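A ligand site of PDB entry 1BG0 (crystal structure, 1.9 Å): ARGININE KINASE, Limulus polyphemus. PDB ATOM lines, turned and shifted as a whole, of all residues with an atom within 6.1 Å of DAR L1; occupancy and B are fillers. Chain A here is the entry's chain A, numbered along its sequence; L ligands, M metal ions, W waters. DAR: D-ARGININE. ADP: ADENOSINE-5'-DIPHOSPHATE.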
ATOM      1  N   SER A  24     -12.883 -15.064  18.185  1.00  0.00           N
ATOM      2  CA  SER A  24     -14.032 -14.843  17.312  1.00  0.00           C
ATOM      3  C   SER A  24     -14.030 -15.789  16.118  1.00  0.00           C
ATOM      4  O   SER A  24     -12.980 -16.286  15.703  1.00  0.00           O
ATOM      5  CB  SER A  24     -14.053 -13.402  16.796  1.00  0.00           C
ATOM      6  OG  SER A  24     -13.032 -13.186  15.838  1.00  0.00           O
ATOM      7  N   SER A  55     -16.722  -4.703  12.347  1.00  0.00           N
ATOM      8  CA  SER A  55     -17.086  -4.876  13.746  1.00  0.00           C
ATOM      9  C   SER A  55     -16.189  -5.885  14.462  1.00  0.00           C
ATOM     10  O   SER A  55     -15.787  -5.670  15.610  1.00  0.00           O
ATOM     11  CB  SER A  55     -18.552  -5.298  13.879  1.00  0.00           C
ATOM     12  OG  SER A  55     -18.938  -5.389  15.240  1.00  0.00           O
ATOM     13  N   ASP A  61     -13.048  -8.816  21.039  1.00  0.00           N
ATOM     14  CA  ASP A  61     -13.738  -9.673  21.994  1.00  0.00           C
ATOM     15  C   ASP A  61     -15.033 -10.239  21.392  1.00  0.00           C
ATOM     16  O   ASP A  61     -15.825 -10.853  22.096  1.00  0.00           O
ATOM     17  CB  ASP A  61     -14.049  -8.899  23.272  1.00  0.00           C
ATOM     18  CG  ASP A  61     -14.835  -7.637  23.007  1.00  0.00           C
ATOM     19  OD1 ASP A  61     -14.801  -7.134  21.864  1.00  0.00           O
ATOM     20  OD2 ASP A  61     -15.485  -7.124  23.943  1.00  0.00           O
ATOM     21  N   SER A  62     -15.231 -10.011  20.101  1.00  0.00           N
ATOM     22  CA  SER A  62     -16.420 -10.494  19.411  1.00  0.00           C
ATOM     23  C   SER A  62     -16.463 -12.012  19.362  1.00  0.00           C
ATOM     24  O   SER A  62     -15.428 -12.670  19.287  1.00  0.00           O
ATOM     25  CB  SER A  62     -16.460  -9.957  17.974  1.00  0.00           C
ATOM     26  OG  SER A  62     -16.632  -8.548  17.936  1.00  0.00           O
ATOM     27  N   GLY A  63     -17.670 -12.575  19.415  1.00  0.00           N
ATOM     28  CA  GLY A  63     -17.819 -14.015  19.354  1.00  0.00           C
ATOM     29  C   GLY A  63     -17.895 -14.448  17.902  1.00  0.00           C
ATOM     30  O   GLY A  63     -17.373 -15.505  17.523  1.00  0.00           O
ATOM     31  N   VAL A  64     -18.546 -13.627  17.083  1.00  0.00           N
ATOM     32  CA  VAL A  64     -18.690 -13.913  15.655  1.00  0.00           C
ATOM     33  C   VAL A  64     -17.866 -12.898  14.875  1.00  0.00           C
ATOM     34  O   VAL A  64     -16.961 -13.267  14.128  1.00  0.00           O
ATOM     35  CB  VAL A  64     -20.163 -13.835  15.238  1.00  0.00           C
ATOM     36  CG1 VAL A  64     -20.312 -14.233  13.780  1.00  0.00           C
ATOM     37  CG2 VAL A  64     -21.000 -14.746  16.132  1.00  0.00           C
ATOM     38  N   GLY A  65     -18.198 -11.619  15.023  1.00  0.00           N
ATOM     39  CA  GLY A  65     -17.445 -10.568  14.362  1.00  0.00           C
ATOM     40  C   GLY A  65     -17.838 -10.071  12.987  1.00  0.00           C
ATOM     41  O   GLY A  65     -17.178  -9.185  12.459  1.00  0.00           O
ATOM     42  N   ILE A  66     -18.895 -10.621  12.387  1.00  0.00           N
ATOM     43  CA  ILE A  66     -19.302 -10.153  11.060  1.00  0.00           C
ATOM     44  C   ILE A  66     -20.798  -9.909  10.928  1.00  0.00           C
ATOM     45  O   ILE A  66     -21.602 -10.436  11.697  1.00  0.00           O
ATOM     46  CB  ILE A  66     -18.862 -11.110   9.936  1.00  0.00           C
ATOM     47  CG1 ILE A  66     -19.614 -12.439  10.049  1.00  0.00           C
ATOM     48  CG2 ILE A  66     -17.353 -11.327   9.998  1.00  0.00           C
ATOM     49  CD1 ILE A  66     -19.389 -13.360   8.861  1.00  0.00           C
ATOM     50  N   TYR A  67     -21.160  -9.079   9.950  1.00  0.00           N
ATOM     51  CA  TYR A  67     -22.548  -8.749   9.671  1.00  0.00           C
ATOM     52  C   TYR A  67     -22.721  -8.599   8.173  1.00  0.00           C
ATOM     53  O   TYR A  67     -21.741  -8.402   7.449  1.00  0.00           O
ATOM     54  CB  TYR A  67     -22.945  -7.418  10.333  1.00  0.00           C
ATOM     55  CG  TYR A  67     -22.956  -7.414  11.846  1.00  0.00           C
ATOM     56  CD1 TYR A  67     -24.113  -7.733  12.554  1.00  0.00           C
ATOM     57  CD2 TYR A  67     -21.842  -7.021  12.563  1.00  0.00           C
ATOM     58  CE1 TYR A  67     -24.149  -7.642  13.936  1.00  0.00           C
ATOM     59  CE2 TYR A  67     -21.864  -6.934  13.948  1.00  0.00           C
ATOM     60  CZ  TYR A  67     -23.027  -7.252  14.620  1.00  0.00           C
ATOM     61  OH  TYR A  67     -23.075  -7.138  15.988  1.00  0.00           O
ATOM     62  N   TYR A  88     -21.261 -21.721  13.787  1.00  0.00           N
ATOM     63  CA  TYR A  88     -22.208 -21.228  14.770  1.00  0.00           C
ATOM     64  C   TYR A  88     -23.495 -22.038  14.935  1.00  0.00           C
ATOM     65  O   TYR A  88     -23.903 -22.352  16.047  1.00  0.00           O
ATOM     66  CB  TYR A  88     -22.565 -19.771  14.496  1.00  0.00           C
ATOM     67  CG  TYR A  88     -23.550 -19.220  15.499  1.00  0.00           C
ATOM     68  CD1 TYR A  88     -23.119 -18.661  16.692  1.00  0.00           C
ATOM     69  CD2 TYR A  88     -24.926 -19.315  15.282  1.00  0.00           C
ATOM     70  CE1 TYR A  88     -24.012 -18.216  17.652  1.00  0.00           C
ATOM     71  CE2 TYR A  88     -25.831 -18.872  16.230  1.00  0.00           C
ATOM     72  CZ  TYR A  88     -25.372 -18.329  17.413  1.00  0.00           C
ATOM     73  OH  TYR A  88     -26.260 -17.916  18.380  1.00  0.00           O
ATOM     74  N   ARG A 125     -38.412 -14.542  20.825  1.00  0.00           N
ATOM     75  CA  ARG A 125     -38.398 -13.475  19.829  1.00  0.00           C
ATOM     76  C   ARG A 125     -37.999 -13.971  18.458  1.00  0.00           C
ATOM     77  O   ARG A 125     -37.340 -15.000  18.313  1.00  0.00           O
ATOM     78  CB  ARG A 125     -37.473 -12.326  20.254  1.00  0.00           C
ATOM     79  CG  ARG A 125     -35.975 -12.669  20.372  1.00  0.00           C
ATOM     80  CD  ARG A 125     -35.241 -12.671  19.032  1.00  0.00           C
ATOM     81  NE  ARG A 125     -33.794 -12.651  19.254  1.00  0.00           N
ATOM     82  CZ  ARG A 125     -32.869 -13.090  18.399  1.00  0.00           C
ATOM     83  NH1 ARG A 125     -33.232 -13.600  17.223  1.00  0.00           N
ATOM     84  NH2 ARG A 125     -31.589 -13.023  18.720  1.00  0.00           N
ATOM     85  N   PHE A 193     -20.662  -3.355  19.323  1.00  0.00           N
ATOM     86  CA  PHE A 193     -20.531  -4.254  18.191  1.00  0.00           C
ATOM     87  C   PHE A 193     -21.356  -3.765  17.000  1.00  0.00           C
ATOM     88  O   PHE A 193     -20.928  -3.893  15.856  1.00  0.00           O
ATOM     89  CB  PHE A 193     -20.946  -5.680  18.578  1.00  0.00           C
ATOM     90  CG  PHE A 193     -20.184  -6.225  19.757  1.00  0.00           C
ATOM     91  CD1 PHE A 193     -20.625  -5.988  21.046  1.00  0.00           C
ATOM     92  CD2 PHE A 193     -19.007  -6.929  19.566  1.00  0.00           C
ATOM     93  CE1 PHE A 193     -19.911  -6.456  22.141  1.00  0.00           C
ATOM     94  CE2 PHE A 193     -18.282  -7.397  20.652  1.00  0.00           C
ATOM     95  CZ  PHE A 193     -18.732  -7.164  21.941  1.00  0.00           C
ATOM     96  N   LEU A 194     -22.521  -3.201  17.291  1.00  0.00           N
ATOM     97  CA  LEU A 194     -23.394  -2.669  16.253  1.00  0.00           C
ATOM     98  C   LEU A 194     -22.871  -1.341  15.717  1.00  0.00           C
ATOM     99  O   LEU A 194     -22.909  -1.071  14.518  1.00  0.00           O
ATOM    100  CB  LEU A 194     -24.823  -2.491  16.787  1.00  0.00           C
ATOM    101  CG  LEU A 194     -25.611  -3.781  17.034  1.00  0.00           C
ATOM    102  CD1 LEU A 194     -26.915  -3.474  17.746  1.00  0.00           C
ATOM    103  CD2 LEU A 194     -25.867  -4.480  15.713  1.00  0.00           C
ATOM    104  N   GLU A 224     -31.197  -3.762  15.707  1.00  0.00           N
ATOM    105  CA  GLU A 224     -30.282  -4.596  14.940  1.00  0.00           C
ATOM    106  C   GLU A 224     -30.934  -5.049  13.634  1.00  0.00           C
ATOM    107  O   GLU A 224     -30.291  -5.112  12.589  1.00  0.00           O
ATOM    108  CB  GLU A 224     -29.840  -5.816  15.765  1.00  0.00           C
ATOM    109  CG  GLU A 224     -28.904  -6.739  15.003  1.00  0.00           C
ATOM    110  CD  GLU A 224     -28.361  -7.859  15.856  1.00  0.00           C
ATOM    111  OE1 GLU A 224     -28.123  -7.638  17.057  1.00  0.00           O
ATOM    112  OE2 GLU A 224     -28.156  -8.970  15.322  1.00  0.00           O
ATOM    113  N   ARG A 228     -38.134  -6.881  15.431  1.00  0.00           N
ATOM    114  CA  ARG A 228     -37.885  -7.947  16.384  1.00  0.00           C
ATOM    115  C   ARG A 228     -39.252  -8.096  17.048  1.00  0.00           C
ATOM    116  O   ARG A 228     -39.741  -7.180  17.694  1.00  0.00           O
ATOM    117  CB  ARG A 228     -36.816  -7.572  17.402  1.00  0.00           C
ATOM    118  CG  ARG A 228     -35.388  -7.631  16.872  1.00  0.00           C
ATOM    119  CD  ARG A 228     -34.988  -9.049  16.442  1.00  0.00           C
ATOM    120  NE  ARG A 228     -33.594  -9.105  16.008  1.00  0.00           N
ATOM    121  CZ  ARG A 228     -32.552  -9.211  16.827  1.00  0.00           C
ATOM    122  NH1 ARG A 228     -32.753  -9.278  18.145  1.00  0.00           N
ATOM    123  NH2 ARG A 228     -31.313  -9.210  16.351  1.00  0.00           N
ATOM    124  N   CYS A 270     -27.342 -10.127  11.281  1.00  0.00           N
ATOM    125  CA  CYS A 270     -26.254 -10.994  11.741  1.00  0.00           C
ATOM    126  C   CYS A 270     -26.536 -12.431  11.326  1.00  0.00           C
ATOM    127  O   CYS A 270     -27.666 -12.914  11.415  1.00  0.00           O
ATOM    128  CB  CYS A 270     -26.116 -10.926  13.264  1.00  0.00           C
ATOM    129  SG  CYS A 270     -24.946 -12.136  13.958  1.00  0.00           S
ATOM    130  N   THR A 272     -26.049 -15.065  12.793  1.00  0.00           N
ATOM    131  CA  THR A 272     -26.514 -15.909  13.900  1.00  0.00           C
ATOM    132  C   THR A 272     -28.030 -15.907  14.024  1.00  0.00           C
ATOM    133  O   THR A 272     -28.602 -16.780  14.682  1.00  0.00           O
ATOM    134  CB  THR A 272     -25.931 -15.462  15.257  1.00  0.00           C
ATOM    135  OG1 THR A 272     -26.450 -14.166  15.598  1.00  0.00           O
ATOM    136  CG2 THR A 272     -24.407 -15.393  15.199  1.00  0.00           C
ATOM    137  N   ASN A 273     -28.684 -14.940  13.399  1.00  0.00           N
ATOM    138  CA  ASN A 273     -30.137 -14.825  13.481  1.00  0.00           C
ATOM    139  C   ASN A 273     -30.921 -15.264  12.252  1.00  0.00           C
ATOM    140  O   ASN A 273     -32.128 -15.012  12.146  1.00  0.00           O
ATOM    141  CB  ASN A 273     -30.524 -13.397  13.873  1.00  0.00           C
ATOM    142  CG  ASN A 273     -30.111 -13.045  15.292  1.00  0.00           C
ATOM    143  OD1 ASN A 273     -30.337 -13.825  16.227  1.00  0.00           O
ATOM    144  ND2 ASN A 273     -29.519 -11.866  15.479  1.00  0.00           N
ATOM    145  N   ARG A 308     -26.286 -15.943  28.673  1.00  0.00           N
ATOM    146  CA  ARG A 308     -26.102 -14.497  28.586  1.00  0.00           C
ATOM    147  C   ARG A 308     -26.388 -13.848  29.936  1.00  0.00           C
ATOM    148  O   ARG A 308     -26.958 -14.484  30.823  1.00  0.00           O
ATOM    149  CB  ARG A 308     -27.015 -13.886  27.522  1.00  0.00           C
ATOM    150  CG  ARG A 308     -26.769 -14.374  26.112  1.00  0.00           C
ATOM    151  CD  ARG A 308     -27.664 -13.651  25.104  1.00  0.00           C
ATOM    152  NE  ARG A 308     -27.473 -14.148  23.749  1.00  0.00           N
ATOM    153  CZ  ARG A 308     -27.883 -13.527  22.648  1.00  0.00           C
ATOM    154  NH1 ARG A 308     -28.506 -12.353  22.743  1.00  0.00           N
ATOM    155  NH2 ARG A 308     -27.656 -14.059  21.455  1.00  0.00           N
ATOM    156  N   GLU A 313     -26.905 -10.152  26.069  1.00  0.00           N
ATOM    157  CA  GLU A 313     -25.567 -10.568  25.674  1.00  0.00           C
ATOM    158  C   GLU A 313     -24.530  -9.520  26.067  1.00  0.00           C
ATOM    159  O   GLU A 313     -24.850  -8.340  26.191  1.00  0.00           O
ATOM    160  CB  GLU A 313     -25.509 -10.808  24.159  1.00  0.00           C
ATOM    161  CG  GLU A 313     -25.909  -9.607  23.329  1.00  0.00           C
ATOM    162  CD  GLU A 313     -25.675  -9.834  21.844  1.00  0.00           C
ATOM    163  OE1 GLU A 313     -25.136 -10.903  21.473  1.00  0.00           O
ATOM    164  OE2 GLU A 313     -26.003  -8.935  21.051  1.00  0.00           O
ATOM    165  N   HIS A 314     -23.300  -9.975  26.288  1.00  0.00           N
ATOM    166  CA  HIS A 314     -22.198  -9.091  26.653  1.00  0.00           C
ATOM    167  C   HIS A 314     -22.339  -8.458  28.034  1.00  0.00           C
ATOM    168  O   HIS A 314     -21.635  -7.502  28.348  1.00  0.00           O
ATOM    169  CB  HIS A 314     -22.001  -8.007  25.583  1.00  0.00           C
ATOM    170  CG  HIS A 314     -21.886  -8.542  24.192  1.00  0.00           C
ATOM    171  ND1 HIS A 314     -22.687  -8.110  23.161  1.00  0.00           N
ATOM    172  CD2 HIS A 314     -21.086  -9.495  23.669  1.00  0.00           C
ATOM    173  CE1 HIS A 314     -22.384  -8.779  22.054  1.00  0.00           C
ATOM    174  NE2 HIS A 314     -21.415  -9.628  22.338  1.00  0.00           N
HETATM  175  N   DAR L   1     -21.358  -9.190  16.728  1.00  0.00           N
HETATM  176  CA  DAR L   1     -21.371  -9.669  18.138  1.00  0.00           C
HETATM  177  CB  DAR L   1     -22.724 -10.300  18.482  1.00  0.00           C
HETATM  178  CG  DAR L   1     -23.165 -11.420  17.548  1.00  0.00           C
HETATM  179  CD  DAR L   1     -24.366 -12.164  18.138  1.00  0.00           C
HETATM  180  NE  DAR L   1     -25.344 -11.232  18.681  1.00  0.00           N
HETATM  181  CZ  DAR L   1     -26.198 -10.523  17.950  1.00  0.00           C
HETATM  182  NH1 DAR L   1     -26.190 -10.659  16.624  1.00  0.00           N
HETATM  183  NH2 DAR L   1     -27.009  -9.653  18.517  1.00  0.00           N
HETATM  184  C   DAR L   1     -20.260 -10.684  18.383  1.00  0.00           C
HETATM  185  O   DAR L   1     -19.642 -11.120  17.390  1.00  0.00           O
HETATM  186  OXT DAR L   1     -20.021 -11.027  19.559  1.00  0.00           O
HETATM  187  PB  ADP L   2     -32.237 -10.292  21.728  1.00  0.00           P
HETATM  188  O1B ADP L   2     -31.764  -9.098  20.982  1.00  0.00           O
HETATM  189  O2B ADP L   2     -33.679 -10.165  22.047  1.00  0.00           O
HETATM  190  O3B ADP L   2     -31.938 -11.535  20.981  1.00  0.00           O
HETATM  191  PA  ADP L   2     -30.413  -9.524  23.928  1.00  0.00           P
HETATM  192  O1A ADP L   2     -29.860  -8.457  23.056  1.00  0.00           O
HETATM  193  O2A ADP L   2     -29.379 -10.412  24.507  1.00  0.00           O
HETATM  194  O3A ADP L   2     -31.458 -10.444  23.143  1.00  0.00           O
HETATM  195  O5' ADP L   2     -31.313  -8.899  25.099  1.00  0.00           O
HETATM  196  C5' ADP L   2     -32.396  -8.039  24.747  1.00  0.00           C
HETATM  197  C4' ADP L   2     -33.302  -7.874  25.961  1.00  0.00           C
HETATM  198  O4' ADP L   2     -34.076  -9.065  26.167  1.00  0.00           O
HETATM  199  C3' ADP L   2     -32.527  -7.635  27.253  1.00  0.00           C
HETATM  200  O3' ADP L   2     -33.116  -6.540  27.959  1.00  0.00           O
HETATM  201  C2' ADP L   2     -32.699  -8.902  28.071  1.00  0.00           C
HETATM  202  O2' ADP L   2     -32.643  -8.601  29.477  1.00  0.00           O
HETATM  203  C1' ADP L   2     -34.071  -9.351  27.578  1.00  0.00           C
HETATM  204  N9  ADP L   2     -34.397 -10.778  27.863  1.00  0.00           N
HETATM  205  C8  ADP L   2     -33.995 -11.886  27.218  1.00  0.00           C
HETATM  206  N7  ADP L   2     -34.608 -12.971  27.700  1.00  0.00           N
HETATM  207  C5  ADP L   2     -35.387 -12.505  28.676  1.00  0.00           C
HETATM  208  C6  ADP L   2     -36.228 -13.273  29.469  1.00  0.00           C
HETATM  209  N6  ADP L   2     -36.419 -14.585  29.297  1.00  0.00           N
HETATM  210  N1  ADP L   2     -36.941 -12.589  30.381  1.00  0.00           N
HETATM  211  C2  ADP L   2     -36.835 -11.262  30.464  1.00  0.00           C
HETATM  212  N3  ADP L   2     -36.033 -10.522  29.703  1.00  0.00           N
HETATM  213  C4  ADP L   2     -35.272 -11.143  28.787  1.00  0.00           C
HETATM  214 MG    MG M   1     -30.053  -7.956  21.031  1.00  0.00          MG
HETATM  215  O   HOH W   1     -21.893 -10.707  14.435  1.00  0.00           O
HETATM  216  O   HOH W   2     -21.282 -13.252  20.755  1.00  0.00           O
HETATM  217  O   HOH W   3     -25.221  -7.157  17.490  1.00  0.00           O
HETATM  218  O   HOH W   4     -18.744  -8.082  16.167  1.00  0.00           O
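NH2 of DAR L1 is in salt-bridge range of OE1 of Glu 224. An oxygen (O) of DAR L1 lies within hydrogen-bond range of the backbone NH (N) of Val 64, 2.8 Å away. OH of Tyr 67 lies within hydrogen-bond range of N of DAR L1 (2.8 Å). O of DAR L1 sits at hydrogen-bond distance from N of Gly 65. The backbone NH (N) of Gly 63 sits at hydrogen-bond distance from an oxygen (OXT) of DAR L1 (2.8 Å). A nitrogen (NE) of DAR L1 lies within salt-bridge range of the side-chain carboxylate (OE1) of Glu 313 (2.8 Å). NH1 of DAR L1 sits at hydrogen-bond distance from SG of Cys 270 (3.3 Å). A ring nitrogen (NE2) of His 314 is in hydrogen-bond range of an oxygen (OXT) of DAR L1 (3.4 Å). The backbone NH of Glu 313 lies within hydrogen-bond range of an oxygen (O2A) of ADP L2 (2.9 Å). NH1 of Arg 308 lies within salt-bridge range of O2A of ADP L2, 2.8 Å away. O3B of ADP L2 is in salt-bridge range of NH1 of Arg 228, at 3.7 Å. The guanidinium group of Arg 125 is in salt-bridge range of an oxygen (O3B) of ADP L2 (2.7 Å).
OE2 of Glu 224 sits at hydrogen-bond distance from ND2 of Asn 273, 3.2 Å away. The guanidinium group (NH2) of Arg 228 lies within salt-bridge range of the side-chain carboxylate (OE2) of Glu 224 (3.3 Å). NH1 of Arg 308 is in salt-bridge range of OE1 of Glu 313 (3.9 Å). SG of Cys 270 lies within hydrogen-bond range of OG1 of Thr 272 (3.0 Å). The side-chain amide nitrogen of Asn 273 sits close to the guanidinium group of Arg 228. The side-chain amide oxygen (OD1) of Asn 273 is in hydrogen-bond range of the guanidinium group (NH2) of Arg 125. OG of Ser 55 is in hydrogen-bond range of O of Phe 193, 2.6 Å away.
Merely in contact with DAR L1: Ser 62, Phe 193, Thr 272 and Asn 273. 12 residues have an atom within 4 Å of DAR L1: Ser 62, Gly 63, Val 64, Gly 65, Tyr 67, Phe 193, Glu 224, Cys 270, Thr 272, Asn 273, Glu 313 and His 314.
Water W1 lies within hydrogen-bond range of O of Ile 66 (2.8 Å), N of DAR L1 (2.8 Å) and SG of Cys 270 (3.4 Å). Water W4 lies within hydrogen-bond range of OG of Ser 62 (2.8 Å), OG of Ser 55 (2.9 Å) and N of DAR L1 (2.9 Å). Water W3 lies within hydrogen-bond range of the side-chain hydroxyl of Tyr 67, the side-chain carboxylate of Glu 224 and a nitrogen (NH2) of DAR L1.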
